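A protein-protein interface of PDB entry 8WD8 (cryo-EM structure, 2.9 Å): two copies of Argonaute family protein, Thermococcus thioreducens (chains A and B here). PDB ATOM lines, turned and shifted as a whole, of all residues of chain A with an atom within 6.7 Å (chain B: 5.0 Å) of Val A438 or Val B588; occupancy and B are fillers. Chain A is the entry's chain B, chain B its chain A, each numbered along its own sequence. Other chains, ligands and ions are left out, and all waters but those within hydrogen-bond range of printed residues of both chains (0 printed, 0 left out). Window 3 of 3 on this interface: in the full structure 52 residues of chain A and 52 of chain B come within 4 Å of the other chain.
NZ of Lys B585 is in salt-bridge range of OD1 of Asp A434, at 3.2 Å. The side-chain amino group (NZ) of Lys B585 lies within salt-bridge range of the side-chain carboxylate (OE2) of Glu A471, 2.4 Å away. The side-chain carboxylate of Asp B586 lies within salt-bridge range of the guanidinium group of Arg A475 (3.0 Å).
The backbone carbonyl oxygen (O) of Lys A435 sits close to the side-chain amide nitrogen (ND2) of Asn A439 (3.3 Å). NE of Arg A475 is in salt-bridge range of OE2 of Glu A471 (3.6 Å).
Among the printed residues, pairs that only touch across the chains: Lys A435 with Phe B626 (3.9 Å), Val A438 with Lys B585 (3.9 Å), Val A438 with Val B588 (3.7 Å), Ile A442 with Val B589 (3.3 Å), Ile A442 with Gly B592 (3.8 Å), Ile A442 with Lys B593 (3.8 Å), Arg A475 with Lys B585 (3.4 Å) and Arg A475 with Val B589 (3.9 Å).
Printed residues of chain B within 4 Å of Val A438: Lys B585 and Val B588. Val B588 touches just one residue of chain A: Val A438 (3.7 Å). Printed residues of chain B within 4 Å of Glu A471: Lys B585. Of the printed residues of chain A, Phe B626 touches Lys A435 (3.9 Å). Of the printed residues of chain A, Val B589 touches Ile A442 (3.3 Å) and Arg A475 (3.9 Å). Ser A441 touches none of the printed residues of chain B. The nearest residue of chain A that does not touch Val B588 is Ile A442 (4.1 Å).
Of the 13 printed residues of chain B, 7 touch a printed residue of chain A. Of the 13 printed residues of chain A, 6 touch a printed residue of chain B. Hydrophobic or aromatic side chains of chain A within 4 Å of the printed part of chain B: Val A438 and Ile A442. Among the printed residues, 11 pairs touch across the chains.
No position is printed for both chains. Of the 11 pairs that touch across the chains among the printed residues, none has its exchanged pair printed and touching as well.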
ATOM      1  N   SER A 433     -18.582 -25.074  -9.279  1.00  0.00           N
ATOM      2  CA  SER A 433     -17.848 -25.381  -8.059  1.00  0.00           C
ATOM      3  C   SER A 433     -16.355 -25.398  -8.356  1.00  0.00           C
ATOM      4  O   SER A 433     -15.923 -25.985  -9.354  1.00  0.00           O
ATOM      5  CB  SER A 433     -18.290 -26.726  -7.481  1.00  0.00           C
ATOM      6  OG  SER A 433     -17.481 -27.100  -6.380  1.00  0.00           O
ATOM      7  N   ASP A 434     -15.571 -24.751  -7.489  1.00  0.00           N
ATOM      8  CA  ASP A 434     -14.128 -24.685  -7.699  1.00  0.00           C
ATOM      9  C   ASP A 434     -13.455 -26.011  -7.364  1.00  0.00           C
ATOM     10  O   ASP A 434     -12.485 -26.408  -8.024  1.00  0.00           O
ATOM     11  CB  ASP A 434     -13.532 -23.556  -6.860  1.00  0.00           C
ATOM     12  CG  ASP A 434     -14.078 -22.194  -7.242  1.00  0.00           C
ATOM     13  OD1 ASP A 434     -13.935 -21.803  -8.420  1.00  0.00           O
ATOM     14  OD2 ASP A 434     -14.653 -21.515  -6.366  1.00  0.00           O
ATOM     15  N   LYS A 435     -13.960 -26.707  -6.339  1.00  0.00           N
ATOM     16  CA  LYS A 435     -13.364 -27.971  -5.915  1.00  0.00           C
ATOM     17  C   LYS A 435     -13.579 -29.066  -6.953  1.00  0.00           C
ATOM     18  O   LYS A 435     -12.695 -29.904  -7.168  1.00  0.00           O
ATOM     19  CB  LYS A 435     -13.942 -28.391  -4.565  1.00  0.00           C
ATOM     20  CG  LYS A 435     -12.960 -29.121  -3.664  1.00  0.00           C
ATOM     21  CD  LYS A 435     -13.586 -29.441  -2.317  1.00  0.00           C
ATOM     22  CE  LYS A 435     -12.831 -30.553  -1.608  1.00  0.00           C
ATOM     23  NZ  LYS A 435     -11.386 -30.231  -1.450  1.00  0.00           N
ATOM     24  N   ASP A 436     -14.737 -29.060  -7.619  1.00  0.00           N
ATOM     25  CA  ASP A 436     -14.998 -30.033  -8.675  1.00  0.00           C
ATOM     26  C   ASP A 436     -14.109 -29.784  -9.888  1.00  0.00           C
ATOM     27  O   ASP A 436     -13.629 -30.735 -10.516  1.00  0.00           O
ATOM     28  CB  ASP A 436     -16.473 -29.991  -9.072  1.00  0.00           C
ATOM     29  CG  ASP A 436     -17.342 -30.850  -8.175  1.00  0.00           C
ATOM     30  OD1 ASP A 436     -16.785 -31.652  -7.396  1.00  0.00           O
ATOM     31  OD2 ASP A 436     -18.582 -30.724  -8.249  1.00  0.00           O
ATOM     32  N   ILE A 437     -13.864 -28.510 -10.211  1.00  0.00           N
ATOM     33  CA  ILE A 437     -12.955 -28.149 -11.300  1.00  0.00           C
ATOM     34  C   ILE A 437     -11.529 -28.588 -10.976  1.00  0.00           C
ATOM     35  O   ILE A 437     -10.827 -29.152 -11.828  1.00  0.00           O
ATOM     36  CB  ILE A 437     -13.046 -26.632 -11.573  1.00  0.00           C
ATOM     37  CG1 ILE A 437     -14.343 -26.299 -12.320  1.00  0.00           C
ATOM     38  CG2 ILE A 437     -11.829 -26.114 -12.341  1.00  0.00           C
ATOM     39  CD1 ILE A 437     -14.430 -24.860 -12.809  1.00  0.00           C
ATOM     40  N   VAL A 438     -11.104 -28.380  -9.723  1.00  0.00           N
ATOM     41  CA  VAL A 438      -9.762 -28.768  -9.287  1.00  0.00           C
ATOM     42  C   VAL A 438      -9.591 -30.287  -9.327  1.00  0.00           C
ATOM     43  O   VAL A 438      -8.581 -30.800  -9.833  1.00  0.00           O
ATOM     44  CB  VAL A 438      -9.488 -28.184  -7.886  1.00  0.00           C
ATOM     45  CG1 VAL A 438      -8.400 -28.954  -7.155  1.00  0.00           C
ATOM     46  CG2 VAL A 438      -9.117 -26.712  -7.991  1.00  0.00           C
ATOM     47  N   ASN A 439     -10.595 -31.028  -8.840  1.00  0.00           N
ATOM     48  CA  ASN A 439     -10.521 -32.488  -8.842  1.00  0.00           C
ATOM     49  C   ASN A 439     -10.574 -33.054 -10.257  1.00  0.00           C
ATOM     50  O   ASN A 439      -9.889 -34.039 -10.561  1.00  0.00           O
ATOM     51  CB  ASN A 439     -11.650 -33.068  -7.990  1.00  0.00           C
ATOM     52  CG  ASN A 439     -11.485 -32.759  -6.515  1.00  0.00           C
ATOM     53  OD1 ASN A 439     -10.403 -32.384  -6.065  1.00  0.00           O
ATOM     54  ND2 ASN A 439     -12.561 -32.916  -5.753  1.00  0.00           N
ATOM     55  N   LEU A 440     -11.361 -32.428 -11.142  1.00  0.00           N
ATOM     56  CA  LEU A 440     -11.405 -32.853 -12.538  1.00  0.00           C
ATOM     57  C   LEU A 440     -10.077 -32.592 -13.239  1.00  0.00           C
ATOM     58  O   LEU A 440      -9.629 -33.408 -14.053  1.00  0.00           O
ATOM     59  CB  LEU A 440     -12.548 -32.139 -13.263  1.00  0.00           C
ATOM     60  CG  LEU A 440     -12.723 -32.417 -14.757  1.00  0.00           C
ATOM     61  CD1 LEU A 440     -13.321 -33.797 -14.980  1.00  0.00           C
ATOM     62  CD2 LEU A 440     -13.576 -31.344 -15.414  1.00  0.00           C
ATOM     63  N   SER A 441      -9.422 -31.472 -12.911  1.00  0.00           N
ATOM     64  CA  SER A 441      -8.105 -31.181 -13.471  1.00  0.00           C
ATOM     65  C   SER A 441      -7.059 -32.183 -12.990  1.00  0.00           C
ATOM     66  O   SER A 441      -6.216 -32.628 -13.779  1.00  0.00           O
ATOM     67  CB  SER A 441      -7.686 -29.756 -13.112  1.00  0.00           C
ATOM     68  OG  SER A 441      -8.211 -28.821 -14.039  1.00  0.00           O
ATOM     69  N   ILE A 442      -7.117 -32.559 -11.706  1.00  0.00           N
ATOM     70  CA  ILE A 442      -6.195 -33.559 -11.158  1.00  0.00           C
ATOM     71  C   ILE A 442      -6.407 -34.915 -11.828  1.00  0.00           C
ATOM     72  O   ILE A 442      -5.444 -35.593 -12.218  1.00  0.00           O
ATOM     73  CB  ILE A 442      -6.352 -33.647  -9.624  1.00  0.00           C
ATOM     74  CG1 ILE A 442      -5.853 -32.371  -8.937  1.00  0.00           C
ATOM     75  CG2 ILE A 442      -5.615 -34.850  -9.050  1.00  0.00           C
ATOM     76  CD1 ILE A 442      -4.537 -31.838  -9.465  1.00  0.00           C
ATOM     77  N   LYS A 443      -7.675 -35.305 -12.015  1.00  0.00           N
ATOM     78  CA  LYS A 443      -7.979 -36.584 -12.655  1.00  0.00           C
ATOM     79  C   LYS A 443      -7.575 -36.595 -14.126  1.00  0.00           C
ATOM     80  O   LYS A 443      -7.106 -37.618 -14.637  1.00  0.00           O
ATOM     81  CB  LYS A 443      -9.466 -36.907 -12.506  1.00  0.00           C
ATOM     82  CG  LYS A 443      -9.881 -37.292 -11.096  1.00  0.00           C
ATOM     83  CD  LYS A 443     -11.234 -37.979 -11.087  1.00  0.00           C
ATOM     84  CE  LYS A 443     -12.362 -36.974 -11.249  1.00  0.00           C
ATOM     85  NZ  LYS A 443     -13.060 -36.711  -9.961  1.00  0.00           N
ATOM     86  N   GLU A 471     -12.354 -20.209 -17.587  1.00  0.00           N
ATOM     87  CA  GLU A 471     -11.555 -20.980 -16.636  1.00  0.00           C
ATOM     88  C   GLU A 471     -11.470 -22.448 -17.041  1.00  0.00           C
ATOM     89  O   GLU A 471     -10.385 -23.044 -17.016  1.00  0.00           O
ATOM     90  CB  GLU A 471     -12.144 -20.844 -15.232  1.00  0.00           C
ATOM     91  CG  GLU A 471     -11.471 -21.710 -14.183  1.00  0.00           C
ATOM     92  CD  GLU A 471     -12.085 -21.543 -12.811  1.00  0.00           C
ATOM     93  OE1 GLU A 471     -13.116 -20.846 -12.699  1.00  0.00           O
ATOM     94  OE2 GLU A 471     -11.539 -22.111 -11.842  1.00  0.00           O
ATOM     95  N   ARG A 475      -8.023 -24.162 -18.320  1.00  0.00           N
ATOM     96  CA  ARG A 475      -7.480 -25.306 -17.596  1.00  0.00           C
ATOM     97  C   ARG A 475      -7.433 -26.559 -18.460  1.00  0.00           C
ATOM     98  O   ARG A 475      -6.614 -27.448 -18.203  1.00  0.00           O
ATOM     99  CB  ARG A 475      -8.297 -25.568 -16.333  1.00  0.00           C
ATOM    100  CG  ARG A 475      -8.053 -24.563 -15.226  1.00  0.00           C
ATOM    101  CD  ARG A 475      -8.593 -25.063 -13.899  1.00  0.00           C
ATOM    102  NE  ARG A 475      -8.715 -23.986 -12.924  1.00  0.00           N
ATOM    103  CZ  ARG A 475      -7.713 -23.522 -12.191  1.00  0.00           C
ATOM    104  NH1 ARG A 475      -6.501 -24.049 -12.263  1.00  0.00           N
ATOM    105  NH2 ARG A 475      -7.933 -22.507 -11.360  1.00  0.00           N
ATOM    106  N   PHE B 584      -4.459 -19.941  -5.252  1.00  0.00           N
ATOM    107  CA  PHE B 584      -4.487 -21.191  -4.505  1.00  0.00           C
ATOM    108  C   PHE B 584      -5.114 -22.322  -5.313  1.00  0.00           C
ATOM    109  O   PHE B 584      -4.780 -23.488  -5.084  1.00  0.00           O
ATOM    110  CB  PHE B 584      -5.212 -20.996  -3.177  1.00  0.00           C
ATOM    111  CG  PHE B 584      -4.286 -20.913  -1.997  1.00  0.00           C
ATOM    112  CD1 PHE B 584      -3.810 -22.065  -1.389  1.00  0.00           C
ATOM    113  CD2 PHE B 584      -3.873 -19.680  -1.512  1.00  0.00           C
ATOM    114  CE1 PHE B 584      -2.950 -21.990  -0.305  1.00  0.00           C
ATOM    115  CE2 PHE B 584      -3.013 -19.598  -0.431  1.00  0.00           C
ATOM    116  CZ  PHE B 584      -2.552 -20.753   0.173  1.00  0.00           C
ATOM    117  N   LYS B 585      -5.971 -22.004  -6.291  1.00  0.00           N
ATOM    118  CA  LYS B 585      -6.547 -23.054  -7.127  1.00  0.00           C
ATOM    119  C   LYS B 585      -5.497 -23.689  -8.039  1.00  0.00           C
ATOM    120  O   LYS B 585      -5.352 -24.918  -8.062  1.00  0.00           O
ATOM    121  CB  LYS B 585      -7.717 -22.502  -7.938  1.00  0.00           C
ATOM    122  CG  LYS B 585      -9.063 -22.846  -7.326  1.00  0.00           C
ATOM    123  CD  LYS B 585     -10.198 -22.623  -8.304  1.00  0.00           C
ATOM    124  CE  LYS B 585     -10.460 -21.147  -8.504  1.00  0.00           C
ATOM    125  NZ  LYS B 585     -11.148 -20.851  -9.788  1.00  0.00           N
ATOM    126  N   ASP B 586      -4.729 -22.873  -8.772  1.00  0.00           N
ATOM    127  CA  ASP B 586      -3.614 -23.459  -9.526  1.00  0.00           C
ATOM    128  C   ASP B 586      -2.466 -23.940  -8.638  1.00  0.00           C
ATOM    129  O   ASP B 586      -1.691 -24.794  -9.078  1.00  0.00           O
ATOM    130  CB  ASP B 586      -3.088 -22.530 -10.631  1.00  0.00           C
ATOM    131  CG  ASP B 586      -4.189 -21.946 -11.505  1.00  0.00           C
ATOM    132  OD1 ASP B 586      -5.136 -21.327 -11.016  1.00  0.00           O
ATOM    133  OD2 ASP B 586      -4.134 -22.191 -12.731  1.00  0.00           O
ATOM    134  N   MET B 587      -2.364 -23.477  -7.385  1.00  0.00           N
ATOM    135  CA  MET B 587      -1.406 -24.096  -6.467  1.00  0.00           C
ATOM    136  C   MET B 587      -1.802 -25.526  -6.122  1.00  0.00           C
ATOM    137  O   MET B 587      -0.958 -26.433  -6.132  1.00  0.00           O
ATOM    138  CB  MET B 587      -1.264 -23.276  -5.186  1.00  0.00           C
ATOM    139  CG  MET B 587      -0.171 -22.237  -5.232  1.00  0.00           C
ATOM    140  SD  MET B 587       0.460 -21.904  -3.578  1.00  0.00           S
ATOM    141  CE  MET B 587       1.018 -23.535  -3.098  1.00  0.00           C
ATOM    142  N   VAL B 588      -3.085 -25.744  -5.811  1.00  0.00           N
ATOM    143  CA  VAL B 588      -3.570 -27.089  -5.505  1.00  0.00           C
ATOM    144  C   VAL B 588      -3.496 -27.975  -6.747  1.00  0.00           C
ATOM    145  O   VAL B 588      -3.120 -29.150  -6.661  1.00  0.00           O
ATOM    146  CB  VAL B 588      -4.993 -27.022  -4.908  1.00  0.00           C
ATOM    147  CG1 VAL B 588      -5.610 -28.403  -4.760  1.00  0.00           C
ATOM    148  CG2 VAL B 588      -4.957 -26.364  -3.541  1.00  0.00           C
ATOM    149  N   VAL B 589      -3.765 -27.399  -7.928  1.00  0.00           N
ATOM    150  CA  VAL B 589      -3.676 -28.155  -9.182  1.00  0.00           C
ATOM    151  C   VAL B 589      -2.232 -28.566  -9.481  1.00  0.00           C
ATOM    152  O   VAL B 589      -1.964 -29.726  -9.826  1.00  0.00           O
ATOM    153  CB  VAL B 589      -4.298 -27.341 -10.335  1.00  0.00           C
ATOM    154  CG1 VAL B 589      -3.887 -27.889 -11.696  1.00  0.00           C
ATOM    155  CG2 VAL B 589      -5.814 -27.357 -10.226  1.00  0.00           C
ATOM    156  N   GLN B 590      -1.276 -27.645  -9.299  1.00  0.00           N
ATOM    157  CA  GLN B 590       0.126 -27.949  -9.572  1.00  0.00           C
ATOM    158  C   GLN B 590       0.696 -28.939  -8.561  1.00  0.00           C
ATOM    159  O   GLN B 590       1.450 -29.852  -8.924  1.00  0.00           O
ATOM    160  CB  GLN B 590       0.943 -26.657  -9.576  1.00  0.00           C
ATOM    161  CG  GLN B 590       2.287 -26.767 -10.273  1.00  0.00           C
ATOM    162  CD  GLN B 590       2.674 -25.490 -10.990  1.00  0.00           C
ATOM    163  OE1 GLN B 590       1.839 -24.613 -11.218  1.00  0.00           O
ATOM    164  NE2 GLN B 590       3.947 -25.376 -11.349  1.00  0.00           N
ATOM    165  N   PHE B 591       0.342 -28.789  -7.284  1.00  0.00           N
ATOM    166  CA  PHE B 591       0.886 -29.705  -6.288  1.00  0.00           C
ATOM    167  C   PHE B 591       0.189 -31.059  -6.313  1.00  0.00           C
ATOM    168  O   PHE B 591       0.792 -32.055  -5.899  1.00  0.00           O
ATOM    169  CB  PHE B 591       0.829 -29.084  -4.887  1.00  0.00           C
ATOM    170  CG  PHE B 591       1.995 -28.166  -4.566  1.00  0.00           C
ATOM    171  CD1 PHE B 591       2.516 -27.291  -5.515  1.00  0.00           C
ATOM    172  CD2 PHE B 591       2.582 -28.201  -3.311  1.00  0.00           C
ATOM    173  CE1 PHE B 591       3.583 -26.464  -5.213  1.00  0.00           C
ATOM    174  CE2 PHE B 591       3.652 -27.375  -3.003  1.00  0.00           C
ATOM    175  CZ  PHE B 591       4.151 -26.507  -3.955  1.00  0.00           C
ATOM    176  N   GLY B 592      -1.049 -31.130  -6.814  1.00  0.00           N
ATOM    177  CA  GLY B 592      -1.679 -32.418  -7.032  1.00  0.00           C
ATOM    178  C   GLY B 592      -1.206 -33.104  -8.292  1.00  0.00           C
ATOM    179  O   GLY B 592      -1.231 -34.336  -8.373  1.00  0.00           O
ATOM    180  N   LYS B 593      -0.770 -32.331  -9.291  1.00  0.00           N
ATOM    181  CA  LYS B 593      -0.110 -32.936 -10.441  1.00  0.00           C
ATOM    182  C   LYS B 593       1.308 -33.375 -10.098  1.00  0.00           C
ATOM    183  O   LYS B 593       1.864 -34.234 -10.790  1.00  0.00           O
ATOM    184  CB  LYS B 593      -0.121 -31.972 -11.635  1.00  0.00           C
ATOM    185  CG  LYS B 593       1.161 -31.190 -11.891  1.00  0.00           C
ATOM    186  CD  LYS B 593       1.147 -30.499 -13.251  1.00  0.00           C
ATOM    187  CE  LYS B 593      -0.125 -29.690 -13.469  1.00  0.00           C
ATOM    188  NZ  LYS B 593      -0.191 -29.115 -14.840  1.00  0.00           N
ATOM    189  N   LEU B 598      -2.932 -31.111  -1.021  1.00  0.00           N
ATOM    190  CA  LEU B 598      -2.780 -29.853  -0.301  1.00  0.00           C
ATOM    191  C   LEU B 598      -3.955 -29.573   0.631  1.00  0.00           C
ATOM    192  O   LEU B 598      -4.344 -28.414   0.813  1.00  0.00           O
ATOM    193  CB  LEU B 598      -2.595 -28.699  -1.287  1.00  0.00           C
ATOM    194  CG  LEU B 598      -1.556 -27.651  -0.886  1.00  0.00           C
ATOM    195  CD1 LEU B 598      -0.172 -28.261  -0.928  1.00  0.00           C
ATOM    196  CD2 LEU B 598      -1.628 -26.433  -1.788  1.00  0.00           C
ATOM    197  N   PHE B 626     -11.127 -25.193   0.937  1.00  0.00           N
ATOM    198  CA  PHE B 626     -10.150 -26.268   0.814  1.00  0.00           C
ATOM    199  C   PHE B 626      -9.644 -26.774   2.159  1.00  0.00           C
ATOM    200  O   PHE B 626      -8.989 -27.820   2.201  1.00  0.00           O
ATOM    201  CB  PHE B 626      -8.967 -25.809  -0.040  1.00  0.00           C
ATOM    202  CG  PHE B 626      -9.279 -25.720  -1.506  1.00  0.00           C
ATOM    203  CD1 PHE B 626      -9.499 -26.869  -2.253  1.00  0.00           C
ATOM    204  CD2 PHE B 626      -9.355 -24.488  -2.139  1.00  0.00           C
ATOM    205  CE1 PHE B 626      -9.787 -26.791  -3.605  1.00  0.00           C
ATOM    206  CE2 PHE B 626      -9.644 -24.401  -3.491  1.00  0.00           C
ATOM    207  CZ  PHE B 626      -9.860 -25.554  -4.224  1.00  0.00           C
ATOM    208  N   ILE B 628      -7.401 -25.302   4.481  1.00  0.00           N
ATOM    209  CA  ILE B 628      -5.979 -25.082   4.708  1.00  0.00           C
ATOM    210  C   ILE B 628      -5.817 -24.022   5.787  1.00  0.00           C
ATOM    211  O   ILE B 628      -6.606 -23.074   5.863  1.00  0.00           O
ATOM    212  CB  ILE B 628      -5.256 -24.659   3.412  1.00  0.00           C
ATOM    213  CG1 ILE B 628      -5.910 -25.307   2.191  1.00  0.00           C
ATOM    214  CG2 ILE B 628      -3.789 -25.036   3.472  1.00  0.00           C
ATOM    215  CD1 ILE B 628      -5.464 -24.707   0.876  1.00  0.00           C
